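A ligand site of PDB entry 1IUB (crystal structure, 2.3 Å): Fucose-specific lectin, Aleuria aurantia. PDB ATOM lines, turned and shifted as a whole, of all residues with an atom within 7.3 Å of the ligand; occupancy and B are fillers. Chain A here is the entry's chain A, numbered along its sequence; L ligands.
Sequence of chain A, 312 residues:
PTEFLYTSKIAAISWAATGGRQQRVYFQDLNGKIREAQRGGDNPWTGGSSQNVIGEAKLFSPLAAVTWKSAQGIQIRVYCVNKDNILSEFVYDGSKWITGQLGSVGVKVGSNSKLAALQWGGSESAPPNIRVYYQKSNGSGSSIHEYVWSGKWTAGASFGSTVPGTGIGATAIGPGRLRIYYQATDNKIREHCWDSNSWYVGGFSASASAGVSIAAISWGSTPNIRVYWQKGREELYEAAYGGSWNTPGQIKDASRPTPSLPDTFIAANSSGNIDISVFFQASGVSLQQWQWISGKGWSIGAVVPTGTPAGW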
ATOM      1  N   TRP A  68      -5.726 -28.059 -16.427  1.00  0.00           N
ATOM      2  CA  TRP A  68      -6.473 -29.319 -16.346  1.00  0.00           C
ATOM      3  C   TRP A  68      -6.287 -29.795 -14.907  1.00  0.00           C
ATOM      4  O   TRP A  68      -5.417 -29.289 -14.188  1.00  0.00           O
ATOM      5  CB  TRP A  68      -5.953 -30.353 -17.360  1.00  0.00           C
ATOM      6  CG  TRP A  68      -4.577 -30.884 -17.080  1.00  0.00           C
ATOM      7  CD1 TRP A  68      -4.254 -31.932 -16.270  1.00  0.00           C
ATOM      8  CD2 TRP A  68      -3.346 -30.345 -17.545  1.00  0.00           C
ATOM      9  NE1 TRP A  68      -2.893 -32.073 -16.194  1.00  0.00           N
ATOM     10  CE2 TRP A  68      -2.308 -31.115 -16.966  1.00  0.00           C
ATOM     11  CE3 TRP A  68      -3.007 -29.289 -18.404  1.00  0.00           C
ATOM     12  CZ2 TRP A  68      -0.949 -30.851 -17.215  1.00  0.00           C
ATOM     13  CZ3 TRP A  68      -1.654 -29.031 -18.647  1.00  0.00           C
ATOM     14  CH2 TRP A  68      -0.643 -29.812 -18.055  1.00  0.00           C
ATOM     15  N   GLN A  75      -3.318 -28.211 -12.528  1.00  0.00           N
ATOM     16  CA  GLN A  75      -2.130 -28.045 -13.359  1.00  0.00           C
ATOM     17  C   GLN A  75      -2.311 -26.811 -14.252  1.00  0.00           C
ATOM     18  O   GLN A  75      -3.358 -26.658 -14.903  1.00  0.00           O
ATOM     19  CB  GLN A  75      -1.938 -29.249 -14.287  1.00  0.00           C
ATOM     20  CG  GLN A  75      -1.554 -30.561 -13.582  1.00  0.00           C
ATOM     21  CD  GLN A  75      -0.223 -30.439 -12.876  1.00  0.00           C
ATOM     22  OE1 GLN A  75       0.762 -29.956 -13.438  1.00  0.00           O
ATOM     23  NE2 GLN A  75      -0.179 -30.885 -11.621  1.00  0.00           N
ATOM     24  N   ILE A  76      -1.317 -25.916 -14.268  1.00  0.00           N
ATOM     25  CA  ILE A  76      -1.392 -24.770 -15.142  1.00  0.00           C
ATOM     26  C   ILE A  76      -0.095 -24.646 -15.914  1.00  0.00           C
ATOM     27  O   ILE A  76       0.988 -24.840 -15.357  1.00  0.00           O
ATOM     28  CB  ILE A  76      -1.605 -23.424 -14.381  1.00  0.00           C
ATOM     29  CG1 ILE A  76      -2.866 -23.469 -13.525  1.00  0.00           C
ATOM     30  CG2 ILE A  76      -1.750 -22.284 -15.397  1.00  0.00           C
ATOM     31  CD1 ILE A  76      -2.958 -22.305 -12.578  1.00  0.00           C
ATOM     32  N   ARG A  77      -0.215 -24.331 -17.205  1.00  0.00           N
ATOM     33  CA  ARG A  77       0.935 -24.104 -18.057  1.00  0.00           C
ATOM     34  C   ARG A  77       0.785 -22.710 -18.704  1.00  0.00           C
ATOM     35  O   ARG A  77      -0.254 -22.398 -19.316  1.00  0.00           O
ATOM     36  CB  ARG A  77       1.041 -25.163 -19.150  1.00  0.00           C
ATOM     37  CG  ARG A  77       1.204 -26.597 -18.636  1.00  0.00           C
ATOM     38  CD  ARG A  77       2.524 -26.782 -17.882  1.00  0.00           C
ATOM     39  NE  ARG A  77       2.700 -28.152 -17.387  1.00  0.00           N
ATOM     40  CZ  ARG A  77       2.154 -28.623 -16.272  1.00  0.00           C
ATOM     41  NH1 ARG A  77       1.382 -27.868 -15.512  1.00  0.00           N
ATOM     42  NH2 ARG A  77       2.391 -29.868 -15.908  1.00  0.00           N
ATOM     43  N   TYR A  79       2.633 -20.001 -21.375  1.00  0.00           N
ATOM     44  CA  TYR A  79       3.636 -19.857 -22.411  1.00  0.00           C
ATOM     45  C   TYR A  79       3.951 -18.381 -22.670  1.00  0.00           C
ATOM     46  O   TYR A  79       3.059 -17.526 -22.620  1.00  0.00           O
ATOM     47  CB  TYR A  79       3.151 -20.546 -23.697  1.00  0.00           C
ATOM     48  CG  TYR A  79       2.890 -22.014 -23.493  1.00  0.00           C
ATOM     49  CD1 TYR A  79       1.606 -22.490 -23.194  1.00  0.00           C
ATOM     50  CD2 TYR A  79       3.952 -22.928 -23.434  1.00  0.00           C
ATOM     51  CE1 TYR A  79       1.391 -23.828 -22.837  1.00  0.00           C
ATOM     52  CE2 TYR A  79       3.751 -24.264 -23.078  1.00  0.00           C
ATOM     53  CZ  TYR A  79       2.470 -24.702 -22.762  1.00  0.00           C
ATOM     54  OH  TYR A  79       2.287 -25.982 -22.308  1.00  0.00           O
ATOM     55  N   GLU A  89       8.173 -21.868 -20.960  1.00  0.00           N
ATOM     56  CA  GLU A  89       6.986 -22.281 -20.233  1.00  0.00           C
ATOM     57  C   GLU A  89       7.075 -22.250 -18.723  1.00  0.00           C
ATOM     58  O   GLU A  89       8.066 -22.688 -18.131  1.00  0.00           O
ATOM     59  CB  GLU A  89       6.659 -23.707 -20.702  1.00  0.00           C
ATOM     60  CG  GLU A  89       5.605 -24.432 -19.915  1.00  0.00           C
ATOM     61  CD  GLU A  89       5.626 -25.941 -20.233  1.00  0.00           C
ATOM     62  OE1 GLU A  89       6.666 -26.590 -19.995  1.00  0.00           O
ATOM     63  OE2 GLU A  89       4.612 -26.468 -20.721  1.00  0.00           O
ATOM     64  N   PHE A  90       6.027 -21.708 -18.087  1.00  0.00           N
ATOM     65  CA  PHE A  90       5.982 -21.708 -16.622  1.00  0.00           C
ATOM     66  C   PHE A  90       4.986 -22.778 -16.259  1.00  0.00           C
ATOM     67  O   PHE A  90       3.957 -22.952 -16.915  1.00  0.00           O
ATOM     68  CB  PHE A  90       5.600 -20.345 -16.067  1.00  0.00           C
ATOM     69  CG  PHE A  90       6.632 -19.287 -16.323  1.00  0.00           C
ATOM     70  CD1 PHE A  90       6.266 -18.072 -16.924  1.00  0.00           C
ATOM     71  CD2 PHE A  90       7.972 -19.506 -16.003  1.00  0.00           C
ATOM     72  CE1 PHE A  90       7.222 -17.082 -17.181  1.00  0.00           C
ATOM     73  CE2 PHE A  90       8.942 -18.514 -16.261  1.00  0.00           C
ATOM     74  CZ  PHE A  90       8.555 -17.298 -16.850  1.00  0.00           C
ATOM     75  N   VAL A  91       5.304 -23.514 -15.212  1.00  0.00           N
ATOM     76  CA  VAL A  91       4.489 -24.633 -14.787  1.00  0.00           C
ATOM     77  C   VAL A  91       3.956 -24.485 -13.382  1.00  0.00           C
ATOM     78  O   VAL A  91       4.718 -24.168 -12.483  1.00  0.00           O
ATOM     79  CB  VAL A  91       5.357 -25.920 -14.822  1.00  0.00           C
ATOM     80  CG1 VAL A  91       4.571 -27.101 -14.271  1.00  0.00           C
ATOM     81  CG2 VAL A  91       5.849 -26.181 -16.231  1.00  0.00           C
ATOM     82  N   ASP A  93       2.605 -26.863 -10.840  1.00  0.00           N
ATOM     83  CA  ASP A  93       2.433 -28.322 -10.686  1.00  0.00           C
ATOM     84  C   ASP A  93       1.415 -28.819  -9.677  1.00  0.00           C
ATOM     85  O   ASP A  93       1.441 -29.995  -9.337  1.00  0.00           O
ATOM     86  CB  ASP A  93       3.773 -28.982 -10.352  1.00  0.00           C
ATOM     87  CG  ASP A  93       4.318 -28.544  -8.999  1.00  0.00           C
ATOM     88  OD1 ASP A  93       3.548 -28.025  -8.150  1.00  0.00           O
ATOM     89  OD2 ASP A  93       5.538 -28.710  -8.789  1.00  0.00           O
ATOM     90  N   ILE A  98       7.085 -23.373 -11.163  1.00  0.00           N
ATOM     91  CA  ILE A  98       8.460 -23.676 -11.567  1.00  0.00           C
ATOM     92  C   ILE A  98       8.560 -23.477 -13.076  1.00  0.00           C
ATOM     93  O   ILE A  98       7.633 -22.997 -13.699  1.00  0.00           O
ATOM     94  CB  ILE A  98       8.820 -25.147 -11.248  1.00  0.00           C
ATOM     95  CG1 ILE A  98       7.871 -26.072 -12.014  1.00  0.00           C
ATOM     96  CG2 ILE A  98       8.699 -25.406  -9.744  1.00  0.00           C
ATOM     97  CD1 ILE A  98       8.165 -27.527 -11.830  1.00  0.00           C
ATOM     98  N   THR A  99       9.693 -23.847 -13.664  1.00  0.00           N
ATOM     99  CA  THR A  99       9.881 -23.682 -15.096  1.00  0.00           C
ATOM    100  C   THR A  99       9.736 -25.020 -15.817  1.00  0.00           C
ATOM    101  O   THR A  99      10.239 -26.043 -15.361  1.00  0.00           O
ATOM    102  CB  THR A  99      11.258 -23.053 -15.371  1.00  0.00           C
ATOM    103  OG1 THR A  99      11.309 -21.785 -14.720  1.00  0.00           O
ATOM    104  CG2 THR A  99      11.493 -22.831 -16.857  1.00  0.00           C
ATOM    105  N   GLY A 100       9.037 -25.002 -16.952  1.00  0.00           N
ATOM    106  CA  GLY A 100       8.830 -26.217 -17.717  1.00  0.00           C
ATOM    107  C   GLY A 100       9.999 -26.540 -18.608  1.00  0.00           C
ATOM    108  O   GLY A 100      10.942 -25.763 -18.707  1.00  0.00           O
ATOM    109  N   GLN A 101       9.910 -27.694 -19.269  1.00  0.00           N
ATOM    110  CA  GLN A 101      10.947 -28.192 -20.159  1.00  0.00           C
ATOM    111  C   GLN A 101      10.956 -27.619 -21.566  1.00  0.00           C
ATOM    112  O   GLN A 101      11.952 -27.778 -22.282  1.00  0.00           O
ATOM    113  CB  GLN A 101      10.843 -29.716 -20.268  1.00  0.00           C
ATOM    114  CG  GLN A 101      10.949 -30.421 -18.934  1.00  0.00           C
ATOM    115  CD  GLN A 101      12.216 -30.020 -18.163  1.00  0.00           C
ATOM    116  OE1 GLN A 101      13.327 -30.452 -18.496  1.00  0.00           O
ATOM    117  NE2 GLN A 101      12.056 -29.162 -17.142  1.00  0.00           N
ATOM    118  N   LEU A 102       9.884 -26.954 -21.970  1.00  0.00           N
ATOM    119  CA  LEU A 102       9.817 -26.433 -23.333  1.00  0.00           C
ATOM    120  C   LEU A 102      10.940 -25.453 -23.708  1.00  0.00           C
ATOM    121  O   LEU A 102      11.401 -25.459 -24.857  1.00  0.00           O
ATOM    122  CB  LEU A 102       8.447 -25.782 -23.590  1.00  0.00           C
ATOM    123  CG  LEU A 102       8.271 -25.157 -24.978  1.00  0.00           C
ATOM    124  CD1 LEU A 102       8.391 -26.214 -26.071  1.00  0.00           C
ATOM    125  CD2 LEU A 102       6.898 -24.477 -25.050  1.00  0.00           C
ATOM    126  N   GLY A 103      11.376 -24.630 -22.756  1.00  0.00           N
ATOM    127  CA  GLY A 103      12.445 -23.694 -23.041  1.00  0.00           C
ATOM    128  C   GLY A 103      13.704 -24.380 -23.565  1.00  0.00           C
ATOM    129  O   GLY A 103      14.309 -23.930 -24.537  1.00  0.00           O
ATOM    130  N   PRO A 127      -2.831 -38.574 -18.981  1.00  0.00           N
ATOM    131  CA  PRO A 127      -1.841 -37.538 -19.281  1.00  0.00           C
ATOM    132  C   PRO A 127      -2.441 -36.512 -20.257  1.00  0.00           C
ATOM    133  O   PRO A 127      -3.284 -36.849 -21.107  1.00  0.00           O
ATOM    134  CB  PRO A 127      -0.694 -38.327 -19.903  1.00  0.00           C
ATOM    135  CG  PRO A 127      -1.435 -39.366 -20.701  1.00  0.00           C
ATOM    136  CD  PRO A 127      -2.550 -39.803 -19.740  1.00  0.00           C
ATOM    137  N   PRO A 128      -2.030 -35.242 -20.144  1.00  0.00           N
ATOM    138  CA  PRO A 128      -2.525 -34.156 -20.999  1.00  0.00           C
ATOM    139  C   PRO A 128      -1.960 -34.217 -22.400  1.00  0.00           C
ATOM    140  O   PRO A 128      -0.899 -34.763 -22.615  1.00  0.00           O
ATOM    141  CB  PRO A 128      -2.049 -32.890 -20.298  1.00  0.00           C
ATOM    142  CG  PRO A 128      -1.464 -33.354 -18.989  1.00  0.00           C
ATOM    143  CD  PRO A 128      -0.999 -34.743 -19.218  1.00  0.00           C
ATOM    144  N   ASN A 129      -2.681 -33.637 -23.340  1.00  0.00           N
ATOM    145  CA  ASN A 129      -2.254 -33.529 -24.725  1.00  0.00           C
ATOM    146  C   ASN A 129      -2.270 -32.017 -24.910  1.00  0.00           C
ATOM    147  O   ASN A 129      -3.337 -31.390 -24.881  1.00  0.00           O
ATOM    148  CB  ASN A 129      -3.266 -34.165 -25.663  1.00  0.00           C
ATOM    149  CG  ASN A 129      -3.283 -35.673 -25.557  1.00  0.00           C
ATOM    150  OD1 ASN A 129      -2.464 -36.360 -26.181  1.00  0.00           O
ATOM    151  ND2 ASN A 129      -4.194 -36.196 -24.772  1.00  0.00           N
ATOM    152  N   ILE A 130      -1.089 -31.429 -25.090  1.00  0.00           N
ATOM    153  CA  ILE A 130      -0.988 -29.987 -25.263  1.00  0.00           C
ATOM    154  C   ILE A 130      -0.497 -29.631 -26.657  1.00  0.00           C
ATOM    155  O   ILE A 130       0.334 -30.328 -27.213  1.00  0.00           O
ATOM    156  CB  ILE A 130      -0.022 -29.391 -24.224  1.00  0.00           C
ATOM    157  CG1 ILE A 130      -0.475 -29.763 -22.820  1.00  0.00           C
ATOM    158  CG2 ILE A 130       0.039 -27.856 -24.379  1.00  0.00           C
ATOM    159  CD1 ILE A 130       0.547 -29.447 -21.725  1.00  0.00           C
ATOM    160  N   TRP A 149       2.879 -31.727 -27.337  1.00  0.00           N
ATOM    161  CA  TRP A 149       3.328 -32.437 -26.170  1.00  0.00           C
ATOM    162  C   TRP A 149       2.440 -33.636 -25.868  1.00  0.00           C
ATOM    163  O   TRP A 149       1.262 -33.474 -25.496  1.00  0.00           O
ATOM    164  CB  TRP A 149       3.353 -31.595 -24.926  1.00  0.00           C
ATOM    165  CG  TRP A 149       4.188 -32.286 -23.864  1.00  0.00           C
ATOM    166  CD1 TRP A 149       5.555 -32.183 -23.680  1.00  0.00           C
ATOM    167  CD2 TRP A 149       3.729 -33.199 -22.861  1.00  0.00           C
ATOM    168  NE1 TRP A 149       5.952 -32.966 -22.625  1.00  0.00           N
ATOM    169  CE2 TRP A 149       4.859 -33.605 -22.103  1.00  0.00           C
ATOM    170  CE3 TRP A 149       2.468 -33.721 -22.528  1.00  0.00           C
ATOM    171  CZ2 TRP A 149       4.771 -34.489 -21.031  1.00  0.00           C
ATOM    172  CZ3 TRP A 149       2.372 -34.602 -21.462  1.00  0.00           C
ATOM    173  CH2 TRP A 149       3.519 -34.985 -20.734  1.00  0.00           C
ATOM    174  N   GLY A 151       3.847 -36.648 -23.920  1.00  0.00           N
ATOM    175  CA  GLY A 151       4.950 -37.358 -23.292  1.00  0.00           C
ATOM    176  C   GLY A 151       6.256 -36.608 -23.507  1.00  0.00           C
ATOM    177  O   GLY A 151       7.137 -36.637 -22.658  1.00  0.00           O
ATOM    178  N   TRP A 153       8.091 -33.052 -26.037  1.00  0.00           N
ATOM    179  CA  TRP A 153       7.830 -31.994 -27.006  1.00  0.00           C
ATOM    180  C   TRP A 153       8.375 -32.360 -28.382  1.00  0.00           C
ATOM    181  O   TRP A 153       9.535 -32.768 -28.498  1.00  0.00           O
ATOM    182  CB  TRP A 153       8.454 -30.641 -26.545  1.00  0.00           C
ATOM    183  CG  TRP A 153       7.736 -29.982 -25.381  1.00  0.00           C
ATOM    184  CD1 TRP A 153       8.124 -29.963 -24.070  1.00  0.00           C
ATOM    185  CD2 TRP A 153       6.480 -29.311 -25.441  1.00  0.00           C
ATOM    186  NE1 TRP A 153       7.182 -29.314 -23.289  1.00  0.00           N
ATOM    187  CE2 TRP A 153       6.155 -28.898 -24.116  1.00  0.00           C
ATOM    188  CE3 TRP A 153       5.585 -28.999 -26.482  1.00  0.00           C
ATOM    189  CZ2 TRP A 153       4.955 -28.195 -23.798  1.00  0.00           C
ATOM    190  CZ3 TRP A 153       4.400 -28.302 -26.170  1.00  0.00           C
ATOM    191  CH2 TRP A 153       4.107 -27.909 -24.829  1.00  0.00           C
HETATM  192  C1  LIG L   1       5.918 -30.878 -17.380  1.00  0.00           C
HETATM  193  C2  LIG L   1       6.560 -29.738 -18.224  1.00  0.00           C
HETATM  194  O1  LIG L   1       7.939 -29.560 -17.867  1.00  0.00           O
HETATM  195  C3  LIG L   1       6.424 -30.130 -19.719  1.00  0.00           C
HETATM  196  O2  LIG L   1       7.040 -29.163 -20.567  1.00  0.00           O
HETATM  197  C4  LIG L   1       4.888 -30.298 -20.045  1.00  0.00           C
HETATM  198  O3  LIG L   1       4.202 -29.064 -19.805  1.00  0.00           O
HETATM  199  C5  LIG L   1       4.316 -31.403 -19.117  1.00  0.00           C
HETATM  200  C6  LIG L   1       2.809 -31.617 -19.271  1.00  0.00           C
HETATM  201  O4  LIG L   1       4.525 -31.051 -17.730  1.00  0.00           O
HETATM  202  O5  LIG L   1       5.980 -30.567 -16.043  1.00  0.00           O
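The side-chain carboxylate of Glu 89 lies within hydrogen-bond range of an oxygen (O2) of the ligand, 2.7 Å away. The indole nitrogen (NE1) of Trp 153 sits at hydrogen-bond distance from an oxygen (O2) of the ligand, 2.7 Å away. O3 of the ligand sits at hydrogen-bond distance from NE of Arg 77, 3.0 Å away. The backbone NH of Gln 101 lies within hydrogen-bond range of an oxygen (O1) of the ligand (3.1 Å).
The backbone carbonyl oxygen (O) of Glu 89 sits at hydrogen-bond distance from the backbone NH (N) of Gly 100, 2.8 Å away. The side-chain carboxylate (OE2) of Glu 89 lies within hydrogen-bond range of the side-chain hydroxyl (OH) of Tyr 79 (2.9 Å). NH2 of Arg 77 is in hydrogen-bond range of OE1 of Gln 75, 3.0 Å away. The backbone NH (N) of Trp 149 sits at hydrogen-bond distance from the backbone carbonyl oxygen (O) of Ile 130 (2.9 Å).
CA of Gly 100 touches O1 of the ligand, at 3.5 Å. Leu 102 touches the ligand. Ile 130 touches the ligand (CD1 to C6, 3.98 Å). Trp 149 touches the ligand. Hydrophobic or aromatic side chains that line the ligand: Ile 130, Trp 149 and Trp 153. Eight residues have an atom within 4 Å of the ligand: Arg 77, Glu 89, Gly 100, Gln 101, Leu 102, Ile 130, Trp 149 and Trp 153. The nearest printed residue that does not touch the ligand is Trp 68 (4.1 Å).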
